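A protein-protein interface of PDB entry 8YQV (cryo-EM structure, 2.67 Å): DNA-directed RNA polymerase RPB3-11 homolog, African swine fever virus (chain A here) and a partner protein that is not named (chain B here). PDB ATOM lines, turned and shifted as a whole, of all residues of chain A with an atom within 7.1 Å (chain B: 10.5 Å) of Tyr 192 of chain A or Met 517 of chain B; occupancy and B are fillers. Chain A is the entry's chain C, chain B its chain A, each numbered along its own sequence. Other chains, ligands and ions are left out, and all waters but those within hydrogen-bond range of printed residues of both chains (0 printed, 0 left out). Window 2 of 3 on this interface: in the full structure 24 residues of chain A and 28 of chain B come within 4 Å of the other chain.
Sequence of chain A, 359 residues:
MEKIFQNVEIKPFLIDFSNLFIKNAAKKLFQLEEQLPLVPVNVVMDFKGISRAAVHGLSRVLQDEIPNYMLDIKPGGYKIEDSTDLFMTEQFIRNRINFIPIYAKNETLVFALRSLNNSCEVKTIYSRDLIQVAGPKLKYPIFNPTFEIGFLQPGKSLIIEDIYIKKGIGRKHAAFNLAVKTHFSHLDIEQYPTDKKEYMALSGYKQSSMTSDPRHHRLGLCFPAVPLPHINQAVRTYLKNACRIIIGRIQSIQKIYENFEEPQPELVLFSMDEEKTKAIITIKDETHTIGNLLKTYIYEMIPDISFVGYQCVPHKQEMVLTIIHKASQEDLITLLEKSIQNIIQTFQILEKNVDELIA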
ATOM      1  N   GLU A 190      -1.718  14.663  20.837  1.00  0.00           N
ATOM      2  CA  GLU A 190      -0.523  13.985  21.300  1.00  0.00           C
ATOM      3  C   GLU A 190      -0.459  12.579  20.719  1.00  0.00           C
ATOM      4  O   GLU A 190      -1.465  12.012  20.296  1.00  0.00           O
ATOM      5  CB  GLU A 190      -0.479  13.925  22.829  1.00  0.00           C
ATOM      6  CG  GLU A 190      -0.998  15.154  23.584  1.00  0.00           C
ATOM      7  CD  GLU A 190      -2.503  15.386  23.454  1.00  0.00           C
ATOM      8  OE1 GLU A 190      -3.211  14.491  22.944  1.00  0.00           O
ATOM      9  OE2 GLU A 190      -2.977  16.468  23.861  1.00  0.00           O
ATOM     10  N   GLN A 191       0.742  12.010  20.707  1.00  0.00           N
ATOM     11  CA  GLN A 191       0.969  10.738  20.043  1.00  0.00           C
ATOM     12  C   GLN A 191       1.720   9.770  20.946  1.00  0.00           C
ATOM     13  O   GLN A 191       2.501  10.166  21.810  1.00  0.00           O
ATOM     14  CB  GLN A 191       1.743  10.920  18.738  1.00  0.00           C
ATOM     15  CG  GLN A 191       0.998  11.701  17.682  1.00  0.00           C
ATOM     16  CD  GLN A 191       1.764  11.785  16.395  1.00  0.00           C
ATOM     17  OE1 GLN A 191       2.840  11.217  16.269  1.00  0.00           O
ATOM     18  NE2 GLN A 191       1.224  12.510  15.431  1.00  0.00           N
ATOM     19  N   TYR A 192       1.465   8.493  20.728  1.00  0.00           N
ATOM     20  CA  TYR A 192       2.155   7.387  21.367  1.00  0.00           C
ATOM     21  C   TYR A 192       3.482   7.122  20.680  1.00  0.00           C
ATOM     22  O   TYR A 192       3.679   7.491  19.519  1.00  0.00           O
ATOM     23  CB  TYR A 192       1.312   6.120  21.295  1.00  0.00           C
ATOM     24  CG  TYR A 192       0.003   6.163  22.023  1.00  0.00           C
ATOM     25  CD1 TYR A 192      -0.048   6.430  23.376  1.00  0.00           C
ATOM     26  CD2 TYR A 192      -1.180   5.881  21.369  1.00  0.00           C
ATOM     27  CE1 TYR A 192      -1.241   6.455  24.049  1.00  0.00           C
ATOM     28  CE2 TYR A 192      -2.379   5.900  22.033  1.00  0.00           C
ATOM     29  CZ  TYR A 192      -2.406   6.186  23.374  1.00  0.00           C
ATOM     30  OH  TYR A 192      -3.603   6.209  24.052  1.00  0.00           O
ATOM     31  N   PRO A 193       4.418   6.478  21.363  1.00  0.00           N
ATOM     32  CA  PRO A 193       5.559   5.897  20.652  1.00  0.00           C
ATOM     33  C   PRO A 193       5.160   4.581  20.006  1.00  0.00           C
ATOM     34  O   PRO A 193       5.033   3.566  20.694  1.00  0.00           O
ATOM     35  CB  PRO A 193       6.599   5.694  21.760  1.00  0.00           C
ATOM     36  CG  PRO A 193       6.085   6.480  22.931  1.00  0.00           C
ATOM     37  CD  PRO A 193       4.609   6.424  22.817  1.00  0.00           C
ATOM     38  N   THR A 194       4.962   4.577  18.692  1.00  0.00           N
ATOM     39  CA  THR A 194       4.441   3.402  18.009  1.00  0.00           C
ATOM     40  C   THR A 194       5.529   2.433  17.576  1.00  0.00           C
ATOM     41  O   THR A 194       5.213   1.406  16.967  1.00  0.00           O
ATOM     42  CB  THR A 194       3.604   3.813  16.800  1.00  0.00           C
ATOM     43  OG1 THR A 194       4.185   4.966  16.181  1.00  0.00           O
ATOM     44  CG2 THR A 194       2.189   4.137  17.233  1.00  0.00           C
ATOM     45  N   ASP A 195       6.798   2.736  17.857  1.00  0.00           N
ATOM     46  CA  ASP A 195       7.835   1.720  17.744  1.00  0.00           C
ATOM     47  C   ASP A 195       7.661   0.626  18.786  1.00  0.00           C
ATOM     48  O   ASP A 195       8.128  -0.496  18.574  1.00  0.00           O
ATOM     49  CB  ASP A 195       9.221   2.353  17.869  1.00  0.00           C
ATOM     50  CG  ASP A 195       9.378   3.172  19.135  1.00  0.00           C
ATOM     51  OD1 ASP A 195       8.384   3.343  19.866  1.00  0.00           O
ATOM     52  OD2 ASP A 195      10.500   3.649  19.398  1.00  0.00           O
ATOM     53  N   LYS A 196       7.008   0.930  19.903  1.00  0.00           N
ATOM     54  CA  LYS A 196       6.654  -0.095  20.872  1.00  0.00           C
ATOM     55  C   LYS A 196       5.626  -1.040  20.270  1.00  0.00           C
ATOM     56  O   LYS A 196       4.727  -0.619  19.541  1.00  0.00           O
ATOM     57  CB  LYS A 196       6.095   0.544  22.141  1.00  0.00           C
ATOM     58  CG  LYS A 196       7.097   1.379  22.919  1.00  0.00           C
ATOM     59  CD  LYS A 196       6.419   2.135  24.053  1.00  0.00           C
ATOM     60  CE  LYS A 196       7.431   2.850  24.934  1.00  0.00           C
ATOM     61  NZ  LYS A 196       8.177   3.906  24.198  1.00  0.00           N
ATOM     62  N   TYR A 199       1.711  -0.530  21.001  1.00  0.00           N
ATOM     63  CA  TYR A 199       0.910   0.454  20.289  1.00  0.00           C
ATOM     64  C   TYR A 199       1.028   0.361  18.778  1.00  0.00           C
ATOM     65  O   TYR A 199       0.429   1.181  18.079  1.00  0.00           O
ATOM     66  CB  TYR A 199       1.311   1.868  20.720  1.00  0.00           C
ATOM     67  CG  TYR A 199       0.947   2.208  22.137  1.00  0.00           C
ATOM     68  CD1 TYR A 199       1.876   2.774  22.991  1.00  0.00           C
ATOM     69  CD2 TYR A 199      -0.324   1.969  22.620  1.00  0.00           C
ATOM     70  CE1 TYR A 199       1.550   3.095  24.281  1.00  0.00           C
ATOM     71  CE2 TYR A 199      -0.661   2.285  23.911  1.00  0.00           C
ATOM     72  CZ  TYR A 199       0.279   2.847  24.738  1.00  0.00           C
ATOM     73  OH  TYR A 199      -0.060   3.163  26.032  1.00  0.00           O
ATOM     74  N   LEU A 202      -2.088   0.623  16.540  1.00  0.00           N
ATOM     75  CA  LEU A 202      -2.912   1.818  16.583  1.00  0.00           C
ATOM     76  C   LEU A 202      -2.295   2.908  15.716  1.00  0.00           C
ATOM     77  O   LEU A 202      -1.119   2.862  15.364  1.00  0.00           O
ATOM     78  CB  LEU A 202      -3.067   2.306  18.018  1.00  0.00           C
ATOM     79  CG  LEU A 202      -3.445   1.277  19.079  1.00  0.00           C
ATOM     80  CD1 LEU A 202      -3.622   1.963  20.410  1.00  0.00           C
ATOM     81  CD2 LEU A 202      -4.689   0.527  18.695  1.00  0.00           C
ATOM     82  N   SER A 203      -3.107   3.905  15.372  1.00  0.00           N
ATOM     83  CA  SER A 203      -2.623   4.977  14.511  1.00  0.00           C
ATOM     84  C   SER A 203      -1.476   5.727  15.169  1.00  0.00           C
ATOM     85  O   SER A 203      -0.479   6.049  14.518  1.00  0.00           O
ATOM     86  CB  SER A 203      -3.756   5.937  14.167  1.00  0.00           C
ATOM     87  OG  SER A 203      -4.055   6.786  15.254  1.00  0.00           O
ATOM     88  N   GLY A 204      -1.595   6.006  16.457  1.00  0.00           N
ATOM     89  CA  GLY A 204      -0.541   6.698  17.159  1.00  0.00           C
ATOM     90  C   GLY A 204      -1.059   7.900  17.906  1.00  0.00           C
ATOM     91  O   GLY A 204      -0.498   8.293  18.927  1.00  0.00           O
ATOM     92  N   TYR A 205      -2.126   8.498  17.400  1.00  0.00           N
ATOM     93  CA  TYR A 205      -2.749   9.617  18.081  1.00  0.00           C
ATOM     94  C   TYR A 205      -3.421   9.150  19.363  1.00  0.00           C
ATOM     95  O   TYR A 205      -3.918   8.028  19.456  1.00  0.00           O
ATOM     96  CB  TYR A 205      -3.767  10.285  17.168  1.00  0.00           C
ATOM     97  CG  TYR A 205      -3.156  11.115  16.070  1.00  0.00           C
ATOM     98  CD1 TYR A 205      -2.510  12.301  16.355  1.00  0.00           C
ATOM     99  CD2 TYR A 205      -3.239  10.721  14.754  1.00  0.00           C
ATOM    100  CE1 TYR A 205      -1.965  13.065  15.364  1.00  0.00           C
ATOM    101  CE2 TYR A 205      -2.698  11.481  13.757  1.00  0.00           C
ATOM    102  CZ  TYR A 205      -2.060  12.653  14.067  1.00  0.00           C
ATOM    103  OH  TYR A 205      -1.509  13.414  13.072  1.00  0.00           O
ATOM    104  N   LYS A 206      -3.431  10.024  20.360  1.00  0.00           N
ATOM    105  CA  LYS A 206      -3.973   9.688  21.668  1.00  0.00           C
ATOM    106  C   LYS A 206      -5.468   9.941  21.779  1.00  0.00           C
ATOM    107  O   LYS A 206      -6.051   9.649  22.825  1.00  0.00           O
ATOM    108  CB  LYS A 206      -3.234  10.461  22.758  1.00  0.00           C
ATOM    109  CG  LYS A 206      -1.921   9.831  23.147  1.00  0.00           C
ATOM    110  CD  LYS A 206      -1.283  10.562  24.301  1.00  0.00           C
ATOM    111  CE  LYS A 206      -0.042   9.840  24.768  1.00  0.00           C
ATOM    112  NZ  LYS A 206       0.624  10.565  25.878  1.00  0.00           N
ATOM    113  N   GLN A 207      -6.100  10.465  20.739  1.00  0.00           N
ATOM    114  CA  GLN A 207      -7.541  10.646  20.699  1.00  0.00           C
ATOM    115  C   GLN A 207      -8.105   9.914  19.495  1.00  0.00           C
ATOM    116  O   GLN A 207      -7.509   9.928  18.415  1.00  0.00           O
ATOM    117  CB  GLN A 207      -7.917  12.121  20.620  1.00  0.00           C
ATOM    118  CG  GLN A 207      -7.239  12.992  21.642  1.00  0.00           C
ATOM    119  CD  GLN A 207      -7.621  14.442  21.495  1.00  0.00           C
ATOM    120  OE1 GLN A 207      -8.509  14.781  20.723  1.00  0.00           O
ATOM    121  NE2 GLN A 207      -6.944  15.310  22.230  1.00  0.00           N
ATOM    122  N   SER A 208      -9.248   9.269  19.682  1.00  0.00           N
ATOM    123  CA  SER A 208      -9.944   8.661  18.562  1.00  0.00           C
ATOM    124  C   SER A 208     -10.418   9.736  17.595  1.00  0.00           C
ATOM    125  O   SER A 208     -10.772  10.845  17.993  1.00  0.00           O
ATOM    126  CB  SER A 208     -11.129   7.843  19.051  1.00  0.00           C
ATOM    127  OG  SER A 208     -11.819   7.262  17.967  1.00  0.00           O
ATOM    128  N   SER A 209     -10.413   9.403  16.307  1.00  0.00           N
ATOM    129  CA  SER A 209     -10.862  10.366  15.313  1.00  0.00           C
ATOM    130  C   SER A 209     -12.360  10.593  15.357  1.00  0.00           C
ATOM    131  O   SER A 209     -12.848  11.499  14.678  1.00  0.00           O
ATOM    132  CB  SER A 209     -10.437   9.924  13.918  1.00  0.00           C
ATOM    133  OG  SER A 209     -10.859   8.605  13.646  1.00  0.00           O
ATOM    134  N   LEU B 509     -17.571  -3.866  15.302  1.00  0.00           N
ATOM    135  CA  LEU B 509     -16.788  -2.730  15.771  1.00  0.00           C
ATOM    136  C   LEU B 509     -17.677  -1.576  16.203  1.00  0.00           C
ATOM    137  O   LEU B 509     -17.367  -0.890  17.178  1.00  0.00           O
ATOM    138  CB  LEU B 509     -15.821  -2.265  14.686  1.00  0.00           C
ATOM    139  CG  LEU B 509     -14.786  -3.234  14.117  1.00  0.00           C
ATOM    140  CD1 LEU B 509     -13.986  -2.561  13.032  1.00  0.00           C
ATOM    141  CD2 LEU B 509     -13.878  -3.772  15.189  1.00  0.00           C
ATOM    142  N   ARG B 512     -19.357  -2.663  19.469  1.00  0.00           N
ATOM    143  CA  ARG B 512     -18.355  -3.010  20.462  1.00  0.00           C
ATOM    144  C   ARG B 512     -18.352  -1.987  21.592  1.00  0.00           C
ATOM    145  O   ARG B 512     -18.409  -0.781  21.360  1.00  0.00           O
ATOM    146  CB  ARG B 512     -16.998  -3.049  19.766  1.00  0.00           C
ATOM    147  CG  ARG B 512     -15.833  -3.464  20.561  1.00  0.00           C
ATOM    148  CD  ARG B 512     -14.615  -3.398  19.677  1.00  0.00           C
ATOM    149  NE  ARG B 512     -14.566  -2.148  18.932  1.00  0.00           N
ATOM    150  CZ  ARG B 512     -13.529  -1.747  18.212  1.00  0.00           C
ATOM    151  NH1 ARG B 512     -12.430  -2.475  18.121  1.00  0.00           N
ATOM    152  NH2 ARG B 512     -13.591  -0.582  17.577  1.00  0.00           N
ATOM    153  N   THR B 513     -18.298  -2.470  22.829  1.00  0.00           N
ATOM    154  CA  THR B 513     -18.397  -1.571  23.975  1.00  0.00           C
ATOM    155  C   THR B 513     -17.128  -0.763  24.212  1.00  0.00           C
ATOM    156  O   THR B 513     -17.206   0.434  24.502  1.00  0.00           O
ATOM    157  CB  THR B 513     -18.737  -2.356  25.244  1.00  0.00           C
ATOM    158  OG1 THR B 513     -19.870  -3.192  25.003  1.00  0.00           O
ATOM    159  CG2 THR B 513     -19.075  -1.410  26.365  1.00  0.00           C
ATOM    160  N   ASN B 514     -15.960  -1.389  24.109  1.00  0.00           N
ATOM    161  CA  ASN B 514     -14.688  -0.726  24.343  1.00  0.00           C
ATOM    162  C   ASN B 514     -13.815  -0.810  23.103  1.00  0.00           C
ATOM    163  O   ASN B 514     -13.652  -1.883  22.519  1.00  0.00           O
ATOM    164  CB  ASN B 514     -13.939  -1.332  25.532  1.00  0.00           C
ATOM    165  CG  ASN B 514     -14.578  -1.001  26.858  1.00  0.00           C
ATOM    166  OD1 ASN B 514     -14.993  -1.889  27.597  1.00  0.00           O
ATOM    167  ND2 ASN B 514     -14.662   0.284  27.168  1.00  0.00           N
ATOM    168  N   THR B 515     -13.277   0.327  22.708  1.00  0.00           N
ATOM    169  CA  THR B 515     -12.258   0.483  21.691  1.00  0.00           C
ATOM    170  C   THR B 515     -10.893   0.490  22.377  1.00  0.00           C
ATOM    171  O   THR B 515     -10.807   0.735  23.581  1.00  0.00           O
ATOM    172  CB  THR B 515     -12.542   1.783  20.928  1.00  0.00           C
ATOM    173  OG1 THR B 515     -13.678   1.593  20.082  1.00  0.00           O
ATOM    174  CG2 THR B 515     -11.385   2.270  20.088  1.00  0.00           C
ATOM    175  N   PRO B 516      -9.805   0.171  21.662  1.00  0.00           N
ATOM    176  CA  PRO B 516      -8.476   0.333  22.268  1.00  0.00           C
ATOM    177  C   PRO B 516      -8.173   1.747  22.743  1.00  0.00           C
ATOM    178  O   PRO B 516      -7.162   1.973  23.409  1.00  0.00           O
ATOM    179  CB  PRO B 516      -7.533  -0.082  21.138  1.00  0.00           C
ATOM    180  CG  PRO B 516      -8.298  -1.059  20.378  1.00  0.00           C
ATOM    181  CD  PRO B 516      -9.732  -0.622  20.422  1.00  0.00           C
ATOM    182  N   MET B 517      -9.041   2.701  22.421  1.00  0.00           N
ATOM    183  CA  MET B 517      -8.910   4.083  22.863  1.00  0.00           C
ATOM    184  C   MET B 517      -9.815   4.378  24.053  1.00  0.00           C
ATOM    185  O   MET B 517     -10.023   5.538  24.409  1.00  0.00           O
ATOM    186  CB  MET B 517      -9.213   5.052  21.721  1.00  0.00           C
ATOM    187  CG  MET B 517      -8.288   4.968  20.522  1.00  0.00           C
ATOM    188  SD  MET B 517      -6.792   5.949  20.730  1.00  0.00           S
ATOM    189  CE  MET B 517      -5.743   4.827  21.641  1.00  0.00           C
ATOM    190  N   GLY B 518     -10.357   3.340  24.675  1.00  0.00           N
ATOM    191  CA  GLY B 518     -11.288   3.532  25.764  1.00  0.00           C
ATOM    192  C   GLY B 518     -12.707   3.210  25.358  1.00  0.00           C
ATOM    193  O   GLY B 518     -12.941   2.251  24.624  1.00  0.00           O
ATOM    194  N   LYS B 519     -13.662   4.004  25.823  1.00  0.00           N
ATOM    195  CA  LYS B 519     -15.055   3.760  25.494  1.00  0.00           C
ATOM    196  C   LYS B 519     -15.315   4.030  24.016  1.00  0.00           C
ATOM    197  O   LYS B 519     -14.730   4.929  23.413  1.00  0.00           O
ATOM    198  CB  LYS B 519     -15.963   4.628  26.362  1.00  0.00           C
ATOM    199  CG  LYS B 519     -17.422   4.256  26.282  1.00  0.00           C
ATOM    200  CD  LYS B 519     -18.278   5.167  27.130  1.00  0.00           C
ATOM    201  CE  LYS B 519     -19.749   4.826  26.970  1.00  0.00           C
ATOM    202  NZ  LYS B 519     -20.631   5.754  27.722  1.00  0.00           N
ATOM    203  N   ASN B 520     -16.202   3.227  23.435  1.00  0.00           N
ATOM    204  CA  ASN B 520     -16.535   3.286  22.015  1.00  0.00           C
ATOM    205  C   ASN B 520     -17.652   4.303  21.820  1.00  0.00           C
ATOM    206  O   ASN B 520     -18.839   3.978  21.800  1.00  0.00           O
ATOM    207  CB  ASN B 520     -16.940   1.905  21.524  1.00  0.00           C
ATOM    208  CG  ASN B 520     -16.977   1.791  20.023  1.00  0.00           C
ATOM    209  OD1 ASN B 520     -16.672   2.734  19.304  1.00  0.00           O
ATOM    210  ND2 ASN B 520     -17.359   0.627  19.539  1.00  0.00           N
ATOM    211  N   VAL B 521     -17.257   5.567  21.673  1.00  0.00           N
ATOM    212  CA  VAL B 521     -18.190   6.677  21.539  1.00  0.00           C
ATOM    213  C   VAL B 521     -17.733   7.587  20.407  1.00  0.00           C
ATOM    214  O   VAL B 521     -16.578   7.568  19.988  1.00  0.00           O
ATOM    215  CB  VAL B 521     -18.334   7.482  22.845  1.00  0.00           C
ATOM    216  CG1 VAL B 521     -19.140   6.708  23.849  1.00  0.00           C
ATOM    217  CG2 VAL B 521     -16.975   7.813  23.405  1.00  0.00           C
ATOM    218  N   MET B 522     -18.667   8.397  19.919  1.00  0.00           N
ATOM    219  CA  MET B 522     -18.391   9.396  18.900  1.00  0.00           C
ATOM    220  C   MET B 522     -19.157  10.663  19.247  1.00  0.00           C
ATOM    221  O   MET B 522     -20.198  10.607  19.898  1.00  0.00           O
ATOM    222  CB  MET B 522     -18.789   8.904  17.507  1.00  0.00           C
ATOM    223  CG  MET B 522     -20.133   8.222  17.461  1.00  0.00           C
ATOM    224  SD  MET B 522     -20.292   7.077  16.090  1.00  0.00           S
ATOM    225  CE  MET B 522     -20.225   5.523  16.968  1.00  0.00           C
ATOM    226  N   LEU B 549     -21.108  12.793  23.612  1.00  0.00           N
ATOM    227  CA  LEU B 549     -20.640  11.535  23.055  1.00  0.00           C
ATOM    228  C   LEU B 549     -21.787  10.541  22.960  1.00  0.00           C
ATOM    229  O   LEU B 549     -22.601  10.425  23.878  1.00  0.00           O
ATOM    230  CB  LEU B 549     -19.517  10.958  23.912  1.00  0.00           C
ATOM    231  CG  LEU B 549     -18.356  11.906  24.204  1.00  0.00           C
ATOM    232  CD1 LEU B 549     -17.393  11.272  25.183  1.00  0.00           C
ATOM    233  CD2 LEU B 549     -17.643  12.287  22.924  1.00  0.00           C
ATOM    234  N   TYR B 643     -18.773   3.532   9.882  1.00  0.00           N
ATOM    235  CA  TYR B 643     -17.982   3.464  11.102  1.00  0.00           C
ATOM    236  C   TYR B 643     -16.543   3.090  10.795  1.00  0.00           C
ATOM    237  O   TYR B 643     -15.607   3.721  11.292  1.00  0.00           O
ATOM    238  CB  TYR B 643     -18.597   2.461  12.073  1.00  0.00           C
ATOM    239  CG  TYR B 643     -17.899   2.430  13.402  1.00  0.00           C
ATOM    240  CD1 TYR B 643     -18.204   3.348  14.383  1.00  0.00           C
ATOM    241  CD2 TYR B 643     -16.915   1.499  13.667  1.00  0.00           C
ATOM    242  CE1 TYR B 643     -17.569   3.327  15.584  1.00  0.00           C
ATOM    243  CE2 TYR B 643     -16.269   1.483  14.868  1.00  0.00           C
ATOM    244  CZ  TYR B 643     -16.601   2.399  15.820  1.00  0.00           C
ATOM    245  OH  TYR B 643     -15.967   2.389  17.033  1.00  0.00           O
ATOM    246  N   ASN B 646     -13.853   5.419   9.560  1.00  0.00           N
ATOM    247  CA  ASN B 646     -13.244   6.258  10.569  1.00  0.00           C
ATOM    248  C   ASN B 646     -12.478   5.459  11.610  1.00  0.00           C
ATOM    249  O   ASN B 646     -11.647   6.035  12.314  1.00  0.00           O
ATOM    250  CB  ASN B 646     -14.324   7.105  11.256  1.00  0.00           C
ATOM    251  CG  ASN B 646     -13.794   8.398  11.779  1.00  0.00           C
ATOM    252  OD1 ASN B 646     -14.533   9.357  11.940  1.00  0.00           O
ATOM    253  ND2 ASN B 646     -12.505   8.441  12.049  1.00  0.00           N
ATOM    254  N   ALA B 647     -12.732   4.160  11.722  1.00  0.00           N
ATOM    255  CA  ALA B 647     -12.033   3.288  12.650  1.00  0.00           C
ATOM    256  C   ALA B 647     -10.939   2.485  11.976  1.00  0.00           C
ATOM    257  O   ALA B 647      -9.956   2.126  12.628  1.00  0.00           O
ATOM    258  CB  ALA B 647     -13.017   2.328  13.314  1.00  0.00           C
ATOM    259  N   ASN B 724      -3.629  -9.993  20.374  1.00  0.00           N
ATOM    260  CA  ASN B 724      -4.523  -9.121  21.117  1.00  0.00           C
ATOM    261  C   ASN B 724      -5.876  -9.160  20.427  1.00  0.00           C
ATOM    262  O   ASN B 724      -5.999  -8.641  19.311  1.00  0.00           O
ATOM    263  CB  ASN B 724      -3.981  -7.700  21.152  1.00  0.00           C
ATOM    264  CG  ASN B 724      -4.797  -6.784  22.030  1.00  0.00           C
ATOM    265  OD1 ASN B 724      -5.785  -7.192  22.630  1.00  0.00           O
ATOM    266  ND2 ASN B 724      -4.386  -5.533  22.109  1.00  0.00           N
ATOM    267  N   GLU B 726      -8.414  -7.423  20.795  1.00  0.00           N
ATOM    268  CA  GLU B 726      -8.994  -6.105  20.606  1.00  0.00           C
ATOM    269  C   GLU B 726      -8.486  -5.401  19.358  1.00  0.00           C
ATOM    270  O   GLU B 726      -9.148  -4.481  18.874  1.00  0.00           O
ATOM    271  CB  GLU B 726      -8.718  -5.233  21.829  1.00  0.00           C
ATOM    272  CG  GLU B 726      -9.828  -4.262  22.156  1.00  0.00           C
ATOM    273  CD  GLU B 726      -9.586  -3.515  23.452  1.00  0.00           C
ATOM    274  OE1 GLU B 726      -8.426  -3.477  23.910  1.00  0.00           O
ATOM    275  OE2 GLU B 726     -10.559  -2.987  24.025  1.00  0.00           O
ATOM    276  N   THR B 727      -7.338  -5.810  18.820  1.00  0.00           N
ATOM    277  CA  THR B 727      -6.772  -5.167  17.647  1.00  0.00           C
ATOM    278  C   THR B 727      -6.463  -6.114  16.503  1.00  0.00           C
ATOM    279  O   THR B 727      -6.371  -5.654  15.363  1.00  0.00           O
ATOM    280  CB  THR B 727      -5.479  -4.418  18.006  1.00  0.00           C
ATOM    281  OG1 THR B 727      -4.492  -5.350  18.456  1.00  0.00           O
ATOM    282  CG2 THR B 727      -5.728  -3.406  19.094  1.00  0.00           C
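OG of Ser 209 of chain A sits at hydrogen-bond distance from O of Asn 646 of chain B, 3.0 Å away.
The backbone carbonyl oxygen of Tyr 205 of chain A sits close to the side-chain sulfur of Met 517 of chain B (3.8 Å).
Printed residues of chain B that touch a printed residue of chain A: Pro 516, Met 517 and Asn 646.
The side-chain hydroxyl of Ser 203 of chain A is in hydrogen-bond range of the backbone NH of Tyr 205 of chain A, 3.4 Å away.
The backbone NH (N) of Tyr 192 of chain A lies within hydrogen-bond range of the backbone carbonyl oxygen (O) of Gly 204 of chain A, 2.7 Å away.
Of the printed residues of chain A, Met 517 of chain B touches Tyr 192, Leu 202 and Tyr 205.
No residue of chain B comes within 4 Å of Gly 204 of chain A.
Lys 206 of chain A touches none of the printed residues of chain B.
Printed residues of chain A within 4 Å of Asn 646 of chain B: Ser 209.
Of the printed residues of chain B, Leu 202 of chain A touches Pro 516 (3.8 Å) and Met 517 (3.8 Å).
Thr 515 of chain B touches none of the printed residues of chain A.
The nearest printed residue of chain A that does not touch Pro 516 of chain B is Tyr 192 of chain A (5.6 Å).
Among the printed residues, merely in contact across the chains: Tyr 192 of chain A with Met 517 of chain B (3.5 Å), Leu 202 of chain A with Met 517 of chain B (3.8 Å) and Leu 202 of chain A with Pro 516 of chain B (3.8 Å).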
